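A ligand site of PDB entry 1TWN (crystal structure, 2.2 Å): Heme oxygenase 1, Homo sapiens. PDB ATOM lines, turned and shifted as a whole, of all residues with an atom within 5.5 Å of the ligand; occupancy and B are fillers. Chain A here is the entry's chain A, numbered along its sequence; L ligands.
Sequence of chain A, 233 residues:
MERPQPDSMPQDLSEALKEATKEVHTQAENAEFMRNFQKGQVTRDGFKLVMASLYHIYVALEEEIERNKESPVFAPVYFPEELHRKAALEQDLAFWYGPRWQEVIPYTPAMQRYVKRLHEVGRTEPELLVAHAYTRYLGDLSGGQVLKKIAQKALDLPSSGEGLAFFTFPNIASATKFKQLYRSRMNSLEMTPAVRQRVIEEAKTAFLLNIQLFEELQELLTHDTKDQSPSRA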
ATOM      1  N   SER A  14      25.384 -10.082 -40.865  1.00  0.00           N
ATOM      2  CA  SER A  14      25.111  -8.854 -40.131  1.00  0.00           C
ATOM      3  C   SER A  14      23.800  -8.229 -40.583  1.00  0.00           C
ATOM      4  O   SER A  14      23.045  -7.667 -39.778  1.00  0.00           O
ATOM      5  CB  SER A  14      26.251  -7.848 -40.326  1.00  0.00           C
ATOM      6  OG  SER A  14      26.286  -7.354 -41.653  1.00  0.00           O
ATOM      7  N   LEU A  17      20.925 -10.503 -39.226  1.00  0.00           N
ATOM      8  CA  LEU A  17      20.676 -10.294 -37.794  1.00  0.00           C
ATOM      9  C   LEU A  17      19.846  -9.027 -37.565  1.00  0.00           C
ATOM     10  O   LEU A  17      18.835  -9.055 -36.872  1.00  0.00           O
ATOM     11  CB  LEU A  17      22.011 -10.192 -37.037  1.00  0.00           C
ATOM     12  CG  LEU A  17      22.817 -11.474 -36.891  1.00  0.00           C
ATOM     13  CD1 LEU A  17      24.190 -11.172 -36.330  1.00  0.00           C
ATOM     14  CD2 LEU A  17      22.077 -12.447 -35.993  1.00  0.00           C
ATOM     15  N   LYS A  18      20.299  -7.930 -38.151  1.00  0.00           N
ATOM     16  CA  LYS A  18      19.612  -6.643 -38.025  1.00  0.00           C
ATOM     17  C   LYS A  18      18.147  -6.752 -38.419  1.00  0.00           C
ATOM     18  O   LYS A  18      17.269  -6.196 -37.747  1.00  0.00           O
ATOM     19  CB  LYS A  18      20.323  -5.608 -38.907  1.00  0.00           C
ATOM     20  CG  LYS A  18      19.815  -4.182 -38.744  1.00  0.00           C
ATOM     21  CD  LYS A  18      20.480  -3.270 -39.765  1.00  0.00           C
ATOM     22  CE  LYS A  18      20.022  -1.825 -39.601  1.00  0.00           C
ATOM     23  NZ  LYS A  18      20.561  -1.207 -38.359  1.00  0.00           N
ATOM     24  N   HIS A  25      13.758  -5.832 -30.956  1.00  0.00           N
ATOM     25  CA  HIS A  25      14.429  -4.607 -30.519  1.00  0.00           C
ATOM     26  C   HIS A  25      13.365  -3.575 -30.146  1.00  0.00           C
ATOM     27  O   HIS A  25      13.545  -2.780 -29.208  1.00  0.00           O
ATOM     28  CB  HIS A  25      15.335  -4.055 -31.635  1.00  0.00           C
ATOM     29  CG  HIS A  25      16.159  -2.875 -31.218  1.00  0.00           C
ATOM     30  ND1 HIS A  25      15.617  -1.625 -31.026  1.00  0.00           N
ATOM     31  CD2 HIS A  25      17.474  -2.772 -30.930  1.00  0.00           C
ATOM     32  CE1 HIS A  25      16.575  -0.792 -30.646  1.00  0.00           C
ATOM     33  NE2 HIS A  25      17.705  -1.459 -30.579  1.00  0.00           N
ATOM     34  N   ALA A  28      11.964  -4.276 -26.810  1.00  0.00           N
ATOM     35  CA  ALA A  28      12.934  -3.857 -25.810  1.00  0.00           C
ATOM     36  C   ALA A  28      12.724  -2.365 -25.571  1.00  0.00           C
ATOM     37  O   ALA A  28      12.710  -1.911 -24.418  1.00  0.00           O
ATOM     38  CB  ALA A  28      14.359  -4.113 -26.305  1.00  0.00           C
ATOM     39  N   GLU A  29      12.543  -1.620 -26.655  1.00  0.00           N
ATOM     40  CA  GLU A  29      12.323  -0.181 -26.547  1.00  0.00           C
ATOM     41  C   GLU A  29      10.979   0.111 -25.892  1.00  0.00           C
ATOM     42  O   GLU A  29      10.869   1.063 -25.115  1.00  0.00           O
ATOM     43  CB  GLU A  29      12.353   0.466 -27.943  1.00  0.00           C
ATOM     44  CG  GLU A  29      13.693   0.371 -28.660  1.00  0.00           C
ATOM     45  CD  GLU A  29      13.669   1.051 -30.021  1.00  0.00           C
ATOM     46  OE1 GLU A  29      13.513   2.291 -30.068  1.00  0.00           O
ATOM     47  OE2 GLU A  29      13.787   0.341 -31.039  1.00  0.00           O
ATOM     48  N   MET A  34      12.282   0.621 -19.950  1.00  0.00           N
ATOM     49  CA  MET A  34      13.023   1.386 -20.959  1.00  0.00           C
ATOM     50  C   MET A  34      12.228   2.582 -21.472  1.00  0.00           C
ATOM     51  O   MET A  34      12.810   3.578 -21.883  1.00  0.00           O
ATOM     52  CB  MET A  34      13.439   0.478 -22.127  1.00  0.00           C
ATOM     53  CG  MET A  34      14.586  -0.462 -21.803  1.00  0.00           C
ATOM     54  SD  MET A  34      16.165   0.388 -21.525  1.00  0.00           S
ATOM     55  CE  MET A  34      16.158   0.604 -19.817  1.00  0.00           C
ATOM     56  N   GLN A  38      13.763   6.227 -21.568  1.00  0.00           N
ATOM     57  CA  GLN A  38      13.789   7.118 -22.718  1.00  0.00           C
ATOM     58  C   GLN A  38      13.085   8.437 -22.406  1.00  0.00           C
ATOM     59  O   GLN A  38      13.560   9.500 -22.804  1.00  0.00           O
ATOM     60  CB  GLN A  38      13.100   6.454 -23.914  1.00  0.00           C
ATOM     61  CG  GLN A  38      13.768   5.166 -24.362  1.00  0.00           C
ATOM     62  CD  GLN A  38      12.993   4.478 -25.472  1.00  0.00           C
ATOM     63  OE1 GLN A  38      12.977   4.941 -26.607  1.00  0.00           O
ATOM     64  NE2 GLN A  38      12.344   3.372 -25.140  1.00  0.00           N
ATOM     65  N   TYR A 114      19.933 -14.881 -17.492  1.00  0.00           N
ATOM     66  CA  TYR A 114      20.728 -14.342 -18.598  1.00  0.00           C
ATOM     67  C   TYR A 114      22.146 -14.938 -18.506  1.00  0.00           C
ATOM     68  O   TYR A 114      22.657 -15.494 -19.480  1.00  0.00           O
ATOM     69  CB  TYR A 114      20.791 -12.816 -18.482  1.00  0.00           C
ATOM     70  CG  TYR A 114      21.160 -12.072 -19.749  1.00  0.00           C
ATOM     71  CD1 TYR A 114      21.952 -12.659 -20.738  1.00  0.00           C
ATOM     72  CD2 TYR A 114      20.771 -10.749 -19.921  1.00  0.00           C
ATOM     73  CE1 TYR A 114      22.349 -11.929 -21.862  1.00  0.00           C
ATOM     74  CE2 TYR A 114      21.157 -10.023 -21.017  1.00  0.00           C
ATOM     75  CZ  TYR A 114      21.942 -10.608 -21.990  1.00  0.00           C
ATOM     76  OH  TYR A 114      22.335  -9.839 -23.070  1.00  0.00           O
ATOM     77  N   TYR A 134      27.234  -9.825 -30.335  1.00  0.00           N
ATOM     78  CA  TYR A 134      26.629  -8.868 -31.258  1.00  0.00           C
ATOM     79  C   TYR A 134      25.577  -8.027 -30.552  1.00  0.00           C
ATOM     80  O   TYR A 134      25.636  -6.797 -30.563  1.00  0.00           O
ATOM     81  CB  TYR A 134      25.971  -9.626 -32.420  1.00  0.00           C
ATOM     82  CG  TYR A 134      24.900  -8.847 -33.148  1.00  0.00           C
ATOM     83  CD1 TYR A 134      25.238  -7.853 -34.074  1.00  0.00           C
ATOM     84  CD2 TYR A 134      23.546  -9.127 -32.936  1.00  0.00           C
ATOM     85  CE1 TYR A 134      24.248  -7.147 -34.767  1.00  0.00           C
ATOM     86  CE2 TYR A 134      22.552  -8.428 -33.617  1.00  0.00           C
ATOM     87  CZ  TYR A 134      22.911  -7.441 -34.532  1.00  0.00           C
ATOM     88  OH  TYR A 134      21.929  -6.761 -35.212  1.00  0.00           O
ATOM     89  N   THR A 135      24.612  -8.699 -29.934  1.00  0.00           N
ATOM     90  CA  THR A 135      23.515  -8.052 -29.221  1.00  0.00           C
ATOM     91  C   THR A 135      23.973  -7.057 -28.158  1.00  0.00           C
ATOM     92  O   THR A 135      23.490  -5.930 -28.115  1.00  0.00           O
ATOM     93  CB  THR A 135      22.609  -9.104 -28.573  1.00  0.00           C
ATOM     94  OG1 THR A 135      22.042  -9.942 -29.593  1.00  0.00           O
ATOM     95  CG2 THR A 135      21.468  -8.443 -27.799  1.00  0.00           C
ATOM     96  N   ARG A 136      24.887  -7.485 -27.289  1.00  0.00           N
ATOM     97  CA  ARG A 136      25.397  -6.621 -26.222  1.00  0.00           C
ATOM     98  C   ARG A 136      26.338  -5.524 -26.719  1.00  0.00           C
ATOM     99  O   ARG A 136      26.045  -4.346 -26.558  1.00  0.00           O
ATOM    100  CB  ARG A 136      26.124  -7.466 -25.169  1.00  0.00           C
ATOM    101  CG  ARG A 136      25.207  -8.073 -24.127  1.00  0.00           C
ATOM    102  CD  ARG A 136      25.245  -7.273 -22.839  1.00  0.00           C
ATOM    103  NE  ARG A 136      24.687  -5.928 -22.976  1.00  0.00           N
ATOM    104  CZ  ARG A 136      23.398  -5.630 -22.840  1.00  0.00           C
ATOM    105  NH1 ARG A 136      22.513  -6.592 -22.586  1.00  0.00           N
ATOM    106  NH2 ARG A 136      22.995  -4.371 -22.926  1.00  0.00           N
ATOM    107  N   LEU A 138      27.312  -4.407 -29.887  1.00  0.00           N
ATOM    108  CA  LEU A 138      26.840  -3.472 -30.906  1.00  0.00           C
ATOM    109  C   LEU A 138      25.672  -2.616 -30.435  1.00  0.00           C
ATOM    110  O   LEU A 138      25.527  -1.470 -30.860  1.00  0.00           O
ATOM    111  CB  LEU A 138      26.466  -4.214 -32.190  1.00  0.00           C
ATOM    112  CG  LEU A 138      27.287  -3.720 -33.388  1.00  0.00           C
ATOM    113  CD1 LEU A 138      28.770  -3.923 -33.089  1.00  0.00           C
ATOM    114  CD2 LEU A 138      26.890  -4.448 -34.645  1.00  0.00           C
ATOM    115  N   GLY A 139      24.841  -3.174 -29.565  1.00  0.00           N
ATOM    116  CA  GLY A 139      23.739  -2.410 -29.032  1.00  0.00           C
ATOM    117  C   GLY A 139      24.218  -1.323 -28.088  1.00  0.00           C
ATOM    118  O   GLY A 139      23.821  -0.162 -28.208  1.00  0.00           O
ATOM    119  N   ASP A 140      25.078  -1.687 -27.143  1.00  0.00           N
ATOM    120  CA  ASP A 140      25.597  -0.727 -26.188  1.00  0.00           C
ATOM    121  C   ASP A 140      26.410   0.359 -26.896  1.00  0.00           C
ATOM    122  O   ASP A 140      26.502   1.486 -26.429  1.00  0.00           O
ATOM    123  CB  ASP A 140      26.462  -1.426 -25.130  1.00  0.00           C
ATOM    124  CG  ASP A 140      25.657  -2.405 -24.280  1.00  0.00           C
ATOM    125  OD1 ASP A 140      24.420  -2.258 -24.202  1.00  0.00           O
ATOM    126  OD2 ASP A 140      26.253  -3.315 -23.675  1.00  0.00           O
ATOM    127  N   SER A 142      25.628   1.509 -29.829  1.00  0.00           N
ATOM    128  CA  SER A 142      24.714   2.280 -30.664  1.00  0.00           C
ATOM    129  C   SER A 142      23.717   3.038 -29.786  1.00  0.00           C
ATOM    130  O   SER A 142      23.798   4.258 -29.638  1.00  0.00           O
ATOM    131  CB  SER A 142      23.959   1.380 -31.632  1.00  0.00           C
ATOM    132  OG  SER A 142      24.835   0.701 -32.512  1.00  0.00           O
ATOM    133  N   GLY A 143      22.767   2.303 -29.222  1.00  0.00           N
ATOM    134  CA  GLY A 143      21.784   2.936 -28.365  1.00  0.00           C
ATOM    135  C   GLY A 143      22.401   3.361 -27.054  1.00  0.00           C
ATOM    136  O   GLY A 143      21.923   4.286 -26.378  1.00  0.00           O
ATOM    137  N   VAL A 146      22.810   7.134 -26.550  1.00  0.00           N
ATOM    138  CA  VAL A 146      21.638   8.005 -26.371  1.00  0.00           C
ATOM    139  C   VAL A 146      21.192   7.884 -24.926  1.00  0.00           C
ATOM    140  O   VAL A 146      20.733   8.857 -24.318  1.00  0.00           O
ATOM    141  CB  VAL A 146      20.440   7.611 -27.293  1.00  0.00           C
ATOM    142  CG1 VAL A 146      20.836   7.704 -28.751  1.00  0.00           C
ATOM    143  CG2 VAL A 146      19.944   6.226 -26.949  1.00  0.00           C
ATOM    144  N   LEU A 147      21.330   6.693 -24.369  1.00  0.00           N
ATOM    145  CA  LEU A 147      20.952   6.431 -22.988  1.00  0.00           C
ATOM    146  C   LEU A 147      21.937   7.131 -22.065  1.00  0.00           C
ATOM    147  O   LEU A 147      21.583   7.547 -20.960  1.00  0.00           O
ATOM    148  CB  LEU A 147      20.942   4.930 -22.725  1.00  0.00           C
ATOM    149  CG  LEU A 147      19.933   4.154 -23.571  1.00  0.00           C
ATOM    150  CD1 LEU A 147      20.073   2.669 -23.337  1.00  0.00           C
ATOM    151  CD2 LEU A 147      18.530   4.638 -23.213  1.00  0.00           C
ATOM    152  N   ARG A 183      30.997  -5.680 -38.474  1.00  0.00           N
ATOM    153  CA  ARG A 183      30.032  -6.313 -39.372  1.00  0.00           C
ATOM    154  C   ARG A 183      30.779  -7.176 -40.381  1.00  0.00           C
ATOM    155  O   ARG A 183      30.375  -8.303 -40.652  1.00  0.00           O
ATOM    156  CB  ARG A 183      29.210  -5.247 -40.103  1.00  0.00           C
ATOM    157  CG  ARG A 183      28.360  -4.406 -39.170  1.00  0.00           C
ATOM    158  CD  ARG A 183      27.172  -3.796 -39.883  1.00  0.00           C
ATOM    159  NE  ARG A 183      26.278  -3.128 -38.939  1.00  0.00           N
ATOM    160  CZ  ARG A 183      26.482  -1.928 -38.425  1.00  0.00           C
ATOM    161  NH1 ARG A 183      27.577  -1.233 -38.750  1.00  0.00           N
ATOM    162  NH2 ARG A 183      25.614  -1.410 -37.570  1.00  0.00           N
ATOM    163  N   ALA A 206      18.540 -13.398 -27.083  1.00  0.00           N
ATOM    164  CA  ALA A 206      19.311 -12.424 -26.303  1.00  0.00           C
ATOM    165  C   ALA A 206      18.404 -11.245 -25.936  1.00  0.00           C
ATOM    166  O   ALA A 206      18.385 -10.820 -24.775  1.00  0.00           O
ATOM    167  CB  ALA A 206      20.515 -11.938 -27.106  1.00  0.00           C
ATOM    168  N   PHE A 207      17.639 -10.741 -26.902  1.00  0.00           N
ATOM    169  CA  PHE A 207      16.735  -9.636 -26.632  1.00  0.00           C
ATOM    170  C   PHE A 207      15.671 -10.034 -25.598  1.00  0.00           C
ATOM    171  O   PHE A 207      15.362  -9.270 -24.675  1.00  0.00           O
ATOM    172  CB  PHE A 207      16.032  -9.162 -27.911  1.00  0.00           C
ATOM    173  CG  PHE A 207      16.888  -8.289 -28.787  1.00  0.00           C
ATOM    174  CD1 PHE A 207      17.767  -8.833 -29.709  1.00  0.00           C
ATOM    175  CD2 PHE A 207      16.840  -6.897 -28.652  1.00  0.00           C
ATOM    176  CE1 PHE A 207      18.577  -8.029 -30.495  1.00  0.00           C
ATOM    177  CE2 PHE A 207      17.642  -6.075 -29.430  1.00  0.00           C
ATOM    178  CZ  PHE A 207      18.525  -6.643 -30.348  1.00  0.00           C
ATOM    179  N   ASN A 210      16.887  -9.817 -22.132  1.00  0.00           N
ATOM    180  CA  ASN A 210      17.001  -8.436 -21.672  1.00  0.00           C
ATOM    181  C   ASN A 210      15.599  -7.930 -21.309  1.00  0.00           C
ATOM    182  O   ASN A 210      15.414  -7.256 -20.298  1.00  0.00           O
ATOM    183  CB  ASN A 210      17.582  -7.545 -22.779  1.00  0.00           C
ATOM    184  CG  ASN A 210      19.101  -7.625 -22.852  1.00  0.00           C
ATOM    185  OD1 ASN A 210      19.804  -6.950 -22.119  1.00  0.00           O
ATOM    186  ND2 ASN A 210      19.601  -8.471 -23.753  1.00  0.00           N
ATOM    187  N   PHE A 214      14.176  -6.371 -17.814  1.00  0.00           N
ATOM    188  CA  PHE A 214      13.534  -5.070 -17.675  1.00  0.00           C
ATOM    189  C   PHE A 214      12.214  -5.208 -16.936  1.00  0.00           C
ATOM    190  O   PHE A 214      11.874  -4.364 -16.096  1.00  0.00           O
ATOM    191  CB  PHE A 214      13.253  -4.442 -19.051  1.00  0.00           C
ATOM    192  CG  PHE A 214      14.498  -4.142 -19.867  1.00  0.00           C
ATOM    193  CD1 PHE A 214      15.724  -3.902 -19.243  1.00  0.00           C
ATOM    194  CD2 PHE A 214      14.422  -4.072 -21.256  1.00  0.00           C
ATOM    195  CE1 PHE A 214      16.855  -3.593 -19.997  1.00  0.00           C
ATOM    196  CE2 PHE A 214      15.547  -3.761 -22.020  1.00  0.00           C
ATOM    197  CZ  PHE A 214      16.770  -3.528 -21.383  1.00  0.00           C
HETATM  198 FE1  LIG L   1      19.462  -0.615 -29.719  1.00  0.00          FE
HETATM  199  N1  LIG L   1      19.816   0.788 -31.086  1.00  0.00           N
HETATM  200  N2  LIG L   1      18.501   0.680 -28.568  1.00  0.00           N
HETATM  201  N3  LIG L   1      19.337  -1.971 -28.268  1.00  0.00           N
HETATM  202  N4  LIG L   1      20.577  -1.874 -30.806  1.00  0.00           N
HETATM  203  C1  LIG L   1      20.509   0.689 -32.291  1.00  0.00           C
HETATM  204  C2  LIG L   1      21.180  -0.450 -32.733  1.00  0.00           C
HETATM  205  C3  LIG L   1      21.230  -1.651 -32.017  1.00  0.00           C
HETATM  206  C4  LIG L   1      18.251   2.032 -28.840  1.00  0.00           C
HETATM  207  C5  LIG L   1      18.667   2.712 -30.018  1.00  0.00           C
HETATM  208  C6  LIG L   1      19.402   2.116 -31.071  1.00  0.00           C
HETATM  209  C7  LIG L   1      18.591  -1.914 -27.101  1.00  0.00           C
HETATM  210  O1  LIG L   1      17.873  -0.794 -26.684  1.00  0.00           O
HETATM  211  C8  LIG L   1      17.838   0.423 -27.370  1.00  0.00           C
HETATM  212  C9  LIG L   1      20.874  -3.206 -30.508  1.00  0.00           C
HETATM  213  C10 LIG L   1      20.601  -3.824 -29.311  1.00  0.00           C
HETATM  214  C11 LIG L   1      19.924  -3.234 -28.244  1.00  0.00           C
HETATM  215  C12 LIG L   1      19.868   2.772 -32.281  1.00  0.00           C
HETATM  216  C13 LIG L   1      19.595   4.195 -32.721  1.00  0.00           C
HETATM  217  C14 LIG L   1      17.404   2.599 -27.803  1.00  0.00           C
HETATM  218  C15 LIG L   1      16.874   4.035 -27.741  1.00  0.00           C
HETATM  219  C16 LIG L   1      17.116   1.611 -26.926  1.00  0.00           C
HETATM  220  C17 LIG L   1      16.195   1.672 -25.884  1.00  0.00           C
HETATM  221  C18 LIG L   1      16.336   2.559 -24.759  1.00  0.00           C
HETATM  222  C19 LIG L   1      18.668  -3.185 -26.356  1.00  0.00           C
HETATM  223  C20 LIG L   1      17.817  -3.623 -25.154  1.00  0.00           C
HETATM  224  C21 LIG L   1      19.539  -3.977 -27.049  1.00  0.00           C
HETATM  225  C22 LIG L   1      19.956  -5.283 -26.752  1.00  0.00           C
HETATM  226  C23 LIG L   1      20.233  -5.841 -25.439  1.00  0.00           C
HETATM  227  C24 LIG L   1      21.683  -3.812 -31.544  1.00  0.00           C
HETATM  228  C25 LIG L   1      22.245  -5.230 -31.562  1.00  0.00           C
HETATM  229  C26 LIG L   1      21.925  -2.867 -32.475  1.00  0.00           C
HETATM  230  C27 LIG L   1      22.765  -3.105 -33.728  1.00  0.00           C
HETATM  231  C28 LIG L   1      21.967  -2.995 -35.031  1.00  0.00           C
HETATM  232  C29 LIG L   1      22.732  -3.515 -36.233  1.00  0.00           C
HETATM  233  O2  LIG L   1      22.864  -4.743 -36.379  1.00  0.00           O
HETATM  234  O3  LIG L   1      23.201  -2.689 -37.043  1.00  0.00           O
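An oxygen (O3) of the ligand is in salt-bridge range of the guanidinium group of Arg 183, at 2.8 Å.
An iron atom (FE1) of the ligand is bound by a ring nitrogen (NE2) of His 25, 2.1 Å away.
OH of Tyr 134 is in hydrogen-bond range of O2 of the ligand.
An oxygen (O3) of the ligand is in salt-bridge range of the side-chain amino group (NZ) of Lys 18, at 3.3 Å.
Merely in contact with the ligand: Asn 210 (3.2 Å), Gly 139 (3.3 Å), Leu 147 (3.4 Å), Ser 142 (3.5 Å), Gly 143 (3.5 Å), Phe 207 (3.6 Å), Thr 135 (3.7 Å), Ala 28 (3.7 Å), Gln 38 (3.7 Å), Arg 136 (3.7 Å), Val 146 (3.9 Å), Phe 214 (3.9 Å), Met 34 (3.9 Å) and Glu 29 (3.96 Å).
Hydrophobic or aromatic side chains within 4 Å of the ligand: His 25, Ala 28, Met 34, Tyr 134, Val 146, Leu 147, Phe 207 and Phe 214.
18 residues have an atom within 4 Å of the ligand: Lys 18, His 25, Ala 28, Glu 29, Met 34, Gln 38, Tyr 134, Thr 135, Arg 136, Gly 139, Ser 142, Gly 143, Val 146, Leu 147, Arg 183, Phe 207, Asn 210 and Phe 214.
The guanidinium group (NH2) of Arg 136 is in salt-bridge range of the side-chain carboxylate (OD1) of Asp 140, at 2.9 Å.
ND1 of His 25 is in hydrogen-bond range of OE2 of Glu 29, 2.7 Å away.
NE2 of Gln 38 sits close to O of Met 34, 3.3 Å away.
The guanidinium group (NH1) of Arg 136 sits at hydrogen-bond distance from the side-chain hydroxyl (OH) of Tyr 114, 3.3 Å away.
O of Ala 206 lies within hydrogen-bond range of ND2 of Asn 210 (2.8 Å).
The side-chain amide nitrogen (ND2) of Asn 210 sits at hydrogen-bond distance from the side-chain hydroxyl (OH) of Tyr 114 (3.1 Å).
The side-chain amide oxygen (OD1) of Asn 210 lies within hydrogen-bond range of the guanidinium group (NH1) of Arg 136.
O of Leu 138 is in hydrogen-bond range of OG of Ser 142 (2.8 Å).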
